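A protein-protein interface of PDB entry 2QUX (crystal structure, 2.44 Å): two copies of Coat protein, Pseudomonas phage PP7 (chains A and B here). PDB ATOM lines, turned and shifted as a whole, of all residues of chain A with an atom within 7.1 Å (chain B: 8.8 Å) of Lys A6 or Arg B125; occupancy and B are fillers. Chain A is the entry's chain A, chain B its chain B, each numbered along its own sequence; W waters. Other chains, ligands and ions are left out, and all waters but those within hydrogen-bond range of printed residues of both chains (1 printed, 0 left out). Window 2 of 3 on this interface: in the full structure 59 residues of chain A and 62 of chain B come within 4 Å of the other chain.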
ATOM      1  N   SER A   3      28.906 -18.950  -1.973  1.00  0.00           N
ATOM      2  CA  SER A   3      28.756 -17.770  -1.067  1.00  0.00           C
ATOM      3  C   SER A   3      28.461 -16.463  -1.821  1.00  0.00           C
ATOM      4  O   SER A   3      27.703 -15.623  -1.313  1.00  0.00           O
ATOM      5  CB  SER A   3      30.014 -17.583  -0.200  1.00  0.00           C
ATOM      6  OG  SER A   3      30.172 -18.627   0.750  1.00  0.00           O
ATOM      7  N   MET A   4      29.038 -16.302  -3.019  1.00  0.00           N
ATOM      8  CA  MET A   4      29.047 -15.006  -3.727  1.00  0.00           C
ATOM      9  C   MET A   4      27.981 -14.793  -4.820  1.00  0.00           C
ATOM     10  O   MET A   4      27.645 -13.637  -5.112  1.00  0.00           O
ATOM     11  CB  MET A   4      30.439 -14.726  -4.286  1.00  0.00           C
ATOM     12  CG  MET A   4      31.449 -14.350  -3.214  1.00  0.00           C
ATOM     13  SD  MET A   4      32.920 -13.581  -3.898  1.00  0.00           S
ATOM     14  CE  MET A   4      32.273 -11.981  -4.364  1.00  0.00           C
ATOM     15  N   SER A   5      27.465 -15.867  -5.424  1.00  0.00           N
ATOM     16  CA  SER A   5      26.225 -15.761  -6.225  1.00  0.00           C
ATOM     17  C   SER A   5      25.076 -15.339  -5.310  1.00  0.00           C
ATOM     18  O   SER A   5      24.980 -15.836  -4.184  1.00  0.00           O
ATOM     19  CB  SER A   5      25.845 -17.083  -6.910  1.00  0.00           C
ATOM     20  OG  SER A   5      26.292 -17.135  -8.251  1.00  0.00           O
ATOM     21  N   LYS A   6      24.232 -14.419  -5.778  1.00  0.00           N
ATOM     22  CA  LYS A   6      23.042 -14.001  -5.017  1.00  0.00           C
ATOM     23  C   LYS A   6      21.983 -15.096  -5.071  1.00  0.00           C
ATOM     24  O   LYS A   6      21.888 -15.811  -6.060  1.00  0.00           O
ATOM     25  CB  LYS A   6      22.470 -12.659  -5.506  1.00  0.00           C
ATOM     26  CG  LYS A   6      23.330 -11.480  -5.043  1.00  0.00           C
ATOM     27  CD  LYS A   6      22.681 -10.121  -5.294  1.00  0.00           C
ATOM     28  CE  LYS A   6      23.146  -9.068  -4.261  1.00  0.00           C
ATOM     29  NZ  LYS A   6      24.573  -9.211  -3.786  1.00  0.00           N
ATOM     30  N   THR A   7      21.227 -15.236  -3.983  1.00  0.00           N
ATOM     31  CA  THR A   7      20.243 -16.291  -3.834  1.00  0.00           C
ATOM     32  C   THR A   7      19.029 -15.871  -3.000  1.00  0.00           C
ATOM     33  O   THR A   7      19.037 -14.870  -2.287  1.00  0.00           O
ATOM     34  CB  THR A   7      20.846 -17.564  -3.127  1.00  0.00           C
ATOM     35  OG1 THR A   7      21.167 -17.253  -1.770  1.00  0.00           O
ATOM     36  CG2 THR A   7      22.107 -18.085  -3.802  1.00  0.00           C
ATOM     37  N   ILE A   8      17.987 -16.679  -3.120  1.00  0.00           N
ATOM     38  CA  ILE A   8      16.894 -16.733  -2.161  1.00  0.00           C
ATOM     39  C   ILE A   8      16.817 -18.190  -1.711  1.00  0.00           C
ATOM     40  O   ILE A   8      16.945 -19.115  -2.532  1.00  0.00           O
ATOM     41  CB  ILE A   8      15.552 -16.194  -2.772  1.00  0.00           C
ATOM     42  CG1 ILE A   8      14.435 -16.248  -1.738  1.00  0.00           C
ATOM     43  CG2 ILE A   8      15.162 -16.933  -4.033  1.00  0.00           C
ATOM     44  CD1 ILE A   8      13.281 -15.309  -2.035  1.00  0.00           C
ATOM     45  N   VAL A   9      16.672 -18.392  -0.409  1.00  0.00           N
ATOM     46  CA  VAL A   9      16.682 -19.735   0.193  1.00  0.00           C
ATOM     47  C   VAL A   9      15.312 -20.015   0.791  1.00  0.00           C
ATOM     48  O   VAL A   9      14.837 -19.255   1.641  1.00  0.00           O
ATOM     49  CB  VAL A   9      17.769 -19.849   1.275  1.00  0.00           C
ATOM     50  CG1 VAL A   9      17.812 -21.256   1.863  1.00  0.00           C
ATOM     51  CG2 VAL A   9      19.135 -19.459   0.680  1.00  0.00           C
ATOM     52  N   THR A  18      17.984 -23.588  -2.322  1.00  0.00           N
ATOM     53  CA  THR A  18      18.628 -22.335  -2.661  1.00  0.00           C
ATOM     54  C   THR A  18      18.372 -22.103  -4.139  1.00  0.00           C
ATOM     55  O   THR A  18      18.701 -22.957  -4.972  1.00  0.00           O
ATOM     56  CB  THR A  18      20.143 -22.422  -2.387  1.00  0.00           C
ATOM     57  OG1 THR A  18      20.342 -22.890  -1.052  1.00  0.00           O
ATOM     58  CG2 THR A  18      20.819 -21.066  -2.568  1.00  0.00           C
ATOM     59  N   LEU A  19      17.751 -20.976  -4.453  1.00  0.00           N
ATOM     60  CA  LEU A  19      17.543 -20.571  -5.834  1.00  0.00           C
ATOM     61  C   LEU A  19      18.632 -19.546  -6.101  1.00  0.00           C
ATOM     62  O   LEU A  19      18.714 -18.554  -5.400  1.00  0.00           O
ATOM     63  CB  LEU A  19      16.136 -19.999  -6.039  1.00  0.00           C
ATOM     64  CG  LEU A  19      15.004 -21.014  -6.232  1.00  0.00           C
ATOM     65  CD1 LEU A  19      14.875 -21.944  -5.052  1.00  0.00           C
ATOM     66  CD2 LEU A  19      13.698 -20.289  -6.471  1.00  0.00           C
ATOM     67  N   THR A  20      19.492 -19.824  -7.070  1.00  0.00           N
ATOM     68  CA  THR A  20      20.626 -18.956  -7.429  1.00  0.00           C
ATOM     69  C   THR A  20      20.201 -18.055  -8.571  1.00  0.00           C
ATOM     70  O   THR A  20      19.549 -18.533  -9.505  1.00  0.00           O
ATOM     71  CB  THR A  20      21.794 -19.820  -7.901  1.00  0.00           C
ATOM     72  OG1 THR A  20      22.110 -20.772  -6.871  1.00  0.00           O
ATOM     73  CG2 THR A  20      22.996 -18.968  -8.238  1.00  0.00           C
ATOM     74  N   GLU A  21      20.556 -16.772  -8.499  1.00  0.00           N
ATOM     75  CA  GLU A  21      20.220 -15.798  -9.555  1.00  0.00           C
ATOM     76  C   GLU A  21      20.978 -16.155 -10.822  1.00  0.00           C
ATOM     77  O   GLU A  21      22.196 -16.324 -10.774  1.00  0.00           O
ATOM     78  CB  GLU A  21      20.602 -14.363  -9.169  1.00  0.00           C
ATOM     79  CG  GLU A  21      20.156 -13.323 -10.204  1.00  0.00           C
ATOM     80  CD  GLU A  21      20.191 -11.893  -9.701  1.00  0.00           C
ATOM     81  OE1 GLU A  21      19.110 -11.330  -9.420  1.00  0.00           O
ATOM     82  OE2 GLU A  21      21.298 -11.318  -9.607  1.00  0.00           O
ATOM     83  N   ILE A  22      20.228 -16.312 -11.913  1.00  0.00           N
ATOM     84  CA  ILE A  22      20.800 -16.629 -13.229  1.00  0.00           C
ATOM     85  C   ILE A  22      20.557 -15.518 -14.253  1.00  0.00           C
ATOM     86  O   ILE A  22      21.157 -15.522 -15.336  1.00  0.00           O
ATOM     87  CB  ILE A  22      20.334 -18.018 -13.761  1.00  0.00           C
ATOM     88  CG1 ILE A  22      18.823 -18.101 -14.000  1.00  0.00           C
ATOM     89  CG2 ILE A  22      20.759 -19.125 -12.794  1.00  0.00           C
ATOM     90  CD1 ILE A  22      18.446 -19.299 -14.843  1.00  0.00           C
ATOM     91  N   GLN A  29      13.922 -10.438 -12.843  1.00  0.00           N
ATOM     92  CA  GLN A  29      14.953 -11.305 -12.236  1.00  0.00           C
ATOM     93  C   GLN A  29      14.528 -12.741 -12.358  1.00  0.00           C
ATOM     94  O   GLN A  29      13.346 -13.031 -12.294  1.00  0.00           O
ATOM     95  CB  GLN A  29      15.178 -11.037 -10.743  1.00  0.00           C
ATOM     96  CG  GLN A  29      15.138  -9.597 -10.295  1.00  0.00           C
ATOM     97  CD  GLN A  29      15.288  -9.502  -8.813  1.00  0.00           C
ATOM     98  OE1 GLN A  29      14.292  -9.429  -8.077  1.00  0.00           O
ATOM     99  NE2 GLN A  29      16.535  -9.547  -8.346  1.00  0.00           N
ATOM    100  N   PHE A  31      15.751 -16.527 -10.696  1.00  0.00           N
ATOM    101  CA  PHE A  31      16.506 -17.409  -9.817  1.00  0.00           C
ATOM    102  C   PHE A  31      16.165 -18.851 -10.200  1.00  0.00           C
ATOM    103  O   PHE A  31      15.005 -19.172 -10.408  1.00  0.00           O
ATOM    104  CB  PHE A  31      16.154 -17.170  -8.326  1.00  0.00           C
ATOM    105  CG  PHE A  31      16.465 -15.787  -7.837  1.00  0.00           C
ATOM    106  CD1 PHE A  31      17.592 -15.552  -7.065  1.00  0.00           C
ATOM    107  CD2 PHE A  31      15.663 -14.711  -8.182  1.00  0.00           C
ATOM    108  CE1 PHE A  31      17.908 -14.283  -6.651  1.00  0.00           C
ATOM    109  CE2 PHE A  31      15.979 -13.435  -7.750  1.00  0.00           C
ATOM    110  CZ  PHE A  31      17.097 -13.227  -6.988  1.00  0.00           C
ATOM    111  N   THR B 110       9.523 -15.453   3.349  1.00  0.00           N
ATOM    112  CA  THR B 110      10.855 -14.850   3.306  1.00  0.00           C
ATOM    113  C   THR B 110      10.815 -13.330   3.500  1.00  0.00           C
ATOM    114  O   THR B 110       9.898 -12.663   3.027  1.00  0.00           O
ATOM    115  CB  THR B 110      11.624 -15.176   2.023  1.00  0.00           C
ATOM    116  OG1 THR B 110      10.963 -14.578   0.898  1.00  0.00           O
ATOM    117  CG2 THR B 110      11.770 -16.698   1.856  1.00  0.00           C
ATOM    118  N   SER B 111      11.789 -12.807   4.253  1.00  0.00           N
ATOM    119  CA  SER B 111      11.902 -11.367   4.475  1.00  0.00           C
ATOM    120  C   SER B 111      12.276 -10.624   3.175  1.00  0.00           C
ATOM    121  O   SER B 111      12.015  -9.432   3.053  1.00  0.00           O
ATOM    122  CB  SER B 111      12.909 -11.063   5.593  1.00  0.00           C
ATOM    123  OG  SER B 111      14.059 -11.879   5.483  1.00  0.00           O
ATOM    124  N   GLN B 112      12.905 -11.332   2.236  1.00  0.00           N
ATOM    125  CA  GLN B 112      13.136 -10.822   0.888  1.00  0.00           C
ATOM    126  C   GLN B 112      11.827 -10.451   0.213  1.00  0.00           C
ATOM    127  O   GLN B 112      11.728  -9.365  -0.322  1.00  0.00           O
ATOM    128  CB  GLN B 112      13.870 -11.845   0.030  1.00  0.00           C
ATOM    129  CG  GLN B 112      15.358 -11.946   0.329  1.00  0.00           C
ATOM    130  CD  GLN B 112      16.075 -12.779  -0.685  1.00  0.00           C
ATOM    131  OE1 GLN B 112      15.870 -12.592  -1.877  1.00  0.00           O
ATOM    132  NE2 GLN B 112      16.939 -13.692  -0.233  1.00  0.00           N
ATOM    133  N   VAL B 113      10.816 -11.328   0.304  1.00  0.00           N
ATOM    134  CA  VAL B 113       9.501 -11.047  -0.271  1.00  0.00           C
ATOM    135  C   VAL B 113       8.755  -9.900   0.431  1.00  0.00           C
ATOM    136  O   VAL B 113       8.149  -9.051  -0.244  1.00  0.00           O
ATOM    137  CB  VAL B 113       8.667 -12.295  -0.394  1.00  0.00           C
ATOM    138  CG1 VAL B 113       7.265 -11.951  -0.795  1.00  0.00           C
ATOM    139  CG2 VAL B 113       9.275 -13.166  -1.444  1.00  0.00           C
ATOM    140  N   GLU B 114       8.833  -9.857   1.763  1.00  0.00           N
ATOM    141  CA  GLU B 114       8.373  -8.681   2.521  1.00  0.00           C
ATOM    142  C   GLU B 114       9.050  -7.362   2.096  1.00  0.00           C
ATOM    143  O   GLU B 114       8.410  -6.316   1.988  1.00  0.00           O
ATOM    144  CB  GLU B 114       8.631  -8.886   4.006  1.00  0.00           C
ATOM    145  CG  GLU B 114       7.942  -7.875   4.914  1.00  0.00           C
ATOM    146  CD  GLU B 114       8.142  -8.168   6.391  1.00  0.00           C
ATOM    147  OE1 GLU B 114       8.827  -9.158   6.741  1.00  0.00           O
ATOM    148  OE2 GLU B 114       7.601  -7.391   7.200  1.00  0.00           O
ATOM    149  N   ASP B 115      10.352  -7.421   1.898  1.00  0.00           N
ATOM    150  CA  ASP B 115      11.136  -6.263   1.462  1.00  0.00           C
ATOM    151  C   ASP B 115      10.688  -5.783   0.085  1.00  0.00           C
ATOM    152  O   ASP B 115      10.639  -4.591  -0.167  1.00  0.00           O
ATOM    153  CB  ASP B 115      12.636  -6.618   1.396  1.00  0.00           C
ATOM    154  CG  ASP B 115      13.479  -5.899   2.430  1.00  0.00           C
ATOM    155  OD1 ASP B 115      13.356  -4.661   2.581  1.00  0.00           O
ATOM    156  OD2 ASP B 115      14.325  -6.580   3.043  1.00  0.00           O
ATOM    157  N   LEU B 116      10.383  -6.732  -0.795  1.00  0.00           N
ATOM    158  CA  LEU B 116       9.882  -6.431  -2.114  1.00  0.00           C
ATOM    159  C   LEU B 116       8.535  -5.710  -2.067  1.00  0.00           C
ATOM    160  O   LEU B 116       8.390  -4.612  -2.596  1.00  0.00           O
ATOM    161  CB  LEU B 116       9.789  -7.716  -2.942  1.00  0.00           C
ATOM    162  CG  LEU B 116       9.571  -7.593  -4.454  1.00  0.00           C
ATOM    163  CD1 LEU B 116      10.566  -6.628  -5.149  1.00  0.00           C
ATOM    164  CD2 LEU B 116       9.705  -8.983  -5.036  1.00  0.00           C
ATOM    165  N   ASN B 119       8.857  -2.479   0.658  1.00  0.00           N
ATOM    166  CA  ASN B 119       9.888  -1.461   0.377  1.00  0.00           C
ATOM    167  C   ASN B 119      10.422  -1.374  -1.063  1.00  0.00           C
ATOM    168  O   ASN B 119      11.305  -0.560  -1.335  1.00  0.00           O
ATOM    169  CB  ASN B 119      11.075  -1.661   1.341  1.00  0.00           C
ATOM    170  CG  ASN B 119      10.649  -1.691   2.800  1.00  0.00           C
ATOM    171  OD1 ASN B 119      10.045  -0.738   3.299  1.00  0.00           O
ATOM    172  ND2 ASN B 119      10.966  -2.786   3.491  1.00  0.00           N
ATOM    173  N   LEU B 120       9.897  -2.199  -1.968  1.00  0.00           N
ATOM    174  CA  LEU B 120      10.348  -2.279  -3.360  1.00  0.00           C
ATOM    175  C   LEU B 120      11.794  -2.746  -3.563  1.00  0.00           C
ATOM    176  O   LEU B 120      12.340  -2.587  -4.642  1.00  0.00           O
ATOM    177  CB  LEU B 120      10.015  -0.986  -4.114  1.00  0.00           C
ATOM    178  CG  LEU B 120       8.559  -0.513  -4.001  1.00  0.00           C
ATOM    179  CD1 LEU B 120       8.263   0.598  -5.010  1.00  0.00           C
ATOM    180  CD2 LEU B 120       7.591  -1.650  -4.204  1.00  0.00           C
ATOM    181  N   VAL B 121      12.350  -3.437  -2.566  1.00  0.00           N
ATOM    182  CA  VAL B 121      13.721  -3.902  -2.607  1.00  0.00           C
ATOM    183  C   VAL B 121      13.778  -5.190  -3.459  1.00  0.00           C
ATOM    184  O   VAL B 121      13.072  -6.156  -3.167  1.00  0.00           O
ATOM    185  CB  VAL B 121      14.286  -4.136  -1.192  1.00  0.00           C
ATOM    186  CG1 VAL B 121      15.754  -4.565  -1.244  1.00  0.00           C
ATOM    187  CG2 VAL B 121      14.147  -2.880  -0.353  1.00  0.00           C
ATOM    188  N   PRO B 122      14.590  -5.191  -4.545  1.00  0.00           N
ATOM    189  CA  PRO B 122      14.713  -6.400  -5.348  1.00  0.00           C
ATOM    190  C   PRO B 122      15.177  -7.609  -4.579  1.00  0.00           C
ATOM    191  O   PRO B 122      15.926  -7.470  -3.597  1.00  0.00           O
ATOM    192  CB  PRO B 122      15.818  -6.046  -6.343  1.00  0.00           C
ATOM    193  CG  PRO B 122      15.808  -4.605  -6.426  1.00  0.00           C
ATOM    194  CD  PRO B 122      15.415  -4.099  -5.104  1.00  0.00           C
ATOM    195  N   LEU B 123      14.773  -8.780  -5.065  1.00  0.00           N
ATOM    196  CA  LEU B 123      15.170 -10.038  -4.473  1.00  0.00           C
ATOM    197  C   LEU B 123      16.664 -10.344  -4.669  1.00  0.00           C
ATOM    198  O   LEU B 123      17.298  -9.829  -5.583  1.00  0.00           O
ATOM    199  CB  LEU B 123      14.347 -11.183  -5.059  1.00  0.00           C
ATOM    200  CG  LEU B 123      12.825 -11.145  -4.995  1.00  0.00           C
ATOM    201  CD1 LEU B 123      12.292 -12.422  -5.672  1.00  0.00           C
ATOM    202  CD2 LEU B 123      12.300 -10.988  -3.568  1.00  0.00           C
ATOM    203  N   GLY B 124      17.199 -11.186  -3.785  1.00  0.00           N
ATOM    204  CA  GLY B 124      18.539 -11.781  -3.904  1.00  0.00           C
ATOM    205  C   GLY B 124      19.451 -11.249  -2.822  1.00  0.00           C
ATOM    206  O   GLY B 124      19.577 -10.035  -2.710  1.00  0.00           O
ATOM    207  N   ARG B 125      20.064 -12.138  -2.022  1.00  0.00           N
ATOM    208  CA  ARG B 125      21.036 -11.740  -0.981  1.00  0.00           C
ATOM    209  C   ARG B 125      22.285 -12.635  -0.989  1.00  0.00           C
ATOM    210  O   ARG B 125      23.271 -12.313  -0.317  1.00  0.00           O
ATOM    211  CB  ARG B 125      20.416 -11.789   0.424  1.00  0.00           C
ATOM    212  CG  ARG B 125      19.149 -10.952   0.655  1.00  0.00           C
ATOM    213  CD  ARG B 125      19.423  -9.468   0.583  1.00  0.00           C
ATOM    214  NE  ARG B 125      18.234  -8.685   0.919  1.00  0.00           N
ATOM    215  CZ  ARG B 125      17.163  -8.491   0.134  1.00  0.00           C
ATOM    216  NH1 ARG B 125      17.086  -9.011  -1.081  1.00  0.00           N
ATOM    217  NH2 ARG B 125      16.136  -7.761   0.588  1.00  0.00           N
ATOM    218  OXT ARG B 125      22.362 -13.696  -1.627  1.00  0.00           O
HETATM  219  O   HOH W   1      23.933 -15.864  -1.496  1.00  0.00           O
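O of Thr A7 is in hydrogen-bond range of NE2 of Gln B112 (3.2 Å).
The backbone carbonyl oxygen (O) of Thr A7 lies within hydrogen-bond range of the backbone NH (N) of Arg B125, 2.9 Å away.
O of Leu B123 sits at hydrogen-bond distance from NE2 of Gln A29.
The backbone carbonyl oxygen (O) of Lys A6 is in hydrogen-bond range of the backbone NH (N) of Glu A21, 2.9 Å away.
O of Ile A8 sits at hydrogen-bond distance from N of Leu A19, 2.8 Å away.
The side-chain carboxylate of Glu A21 is in hydrogen-bond range of the side-chain amide nitrogen of Gln A29 (3.3 Å).
OE1 of Gln B112 sits at hydrogen-bond distance from N of Gly B124 (2.7 Å).
OD2 of Asp B115 lies within salt-bridge range of NH2 of Arg B125 (3.3 Å).
NH1 of Arg B125 sits at hydrogen-bond distance from O of Pro B122 (3.2 Å).
Among the printed residues, pairs that only touch across the chains: Lys A6 with Arg B125 (3.5 Å), Thr A7 with Gly B124 (3.5 Å), Ile A8 with Thr B110 (3.8 Å), Ile A8 with Gln B112 (3.6 Å), Val A9 with Thr B110 (3.999 Å), Phe A31 with Leu B123 (3.7 Å) and Phe A31 with Gly B124 (3.7 Å).
No residue of chain B comes within 4 Å of Ser A5.
Of the printed residues of chain B, Lys A6 touches Arg B125 (3.5 Å).
Thr A7 touches three residues of chain B.
Printed residues of chain B within 4 Å of Ile A8: Thr B110 and Gln B112.
Thr A20 touches none of the printed residues of chain B.
Of the printed residues of chain B, Phe A31 touches Leu B123 and Gly B124.
Printed residues of chain A within 4 Å of Arg B125: Lys A6 and Thr A7.
The nearest residue of chain A that does not touch Arg B125 is Ser A5 (4.2 Å).
Of the 14 printed residues of chain B, 5 touch a printed residue of chain A.
Hydrophobic or aromatic side chains of chain B within 4 Å of the printed part of chain A: Leu B123.
Along chain B the printed residues that touch a printed residue of chain A span positions 110 to 125.
Of the 14 printed residues of chain A, 6 touch a printed residue of chain B.
Hydrophobic or aromatic side chains of chain A within 4 Å of the printed part of chain B: Ile A8 and Phe A31.
Among the printed residues, no Asp or Glu carboxylate lies within 4 Å of a Lys or Arg side-chain nitrogen of the other chain.
No position is printed for both chains.
Of the 10 pairs that touch across the chains among the printed residues, none has its exchanged pair printed and touching as well.
Water W1 lies within hydrogen-bond range of OXT of Arg B125, O of Ser A5 and OG1 of Thr A7.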
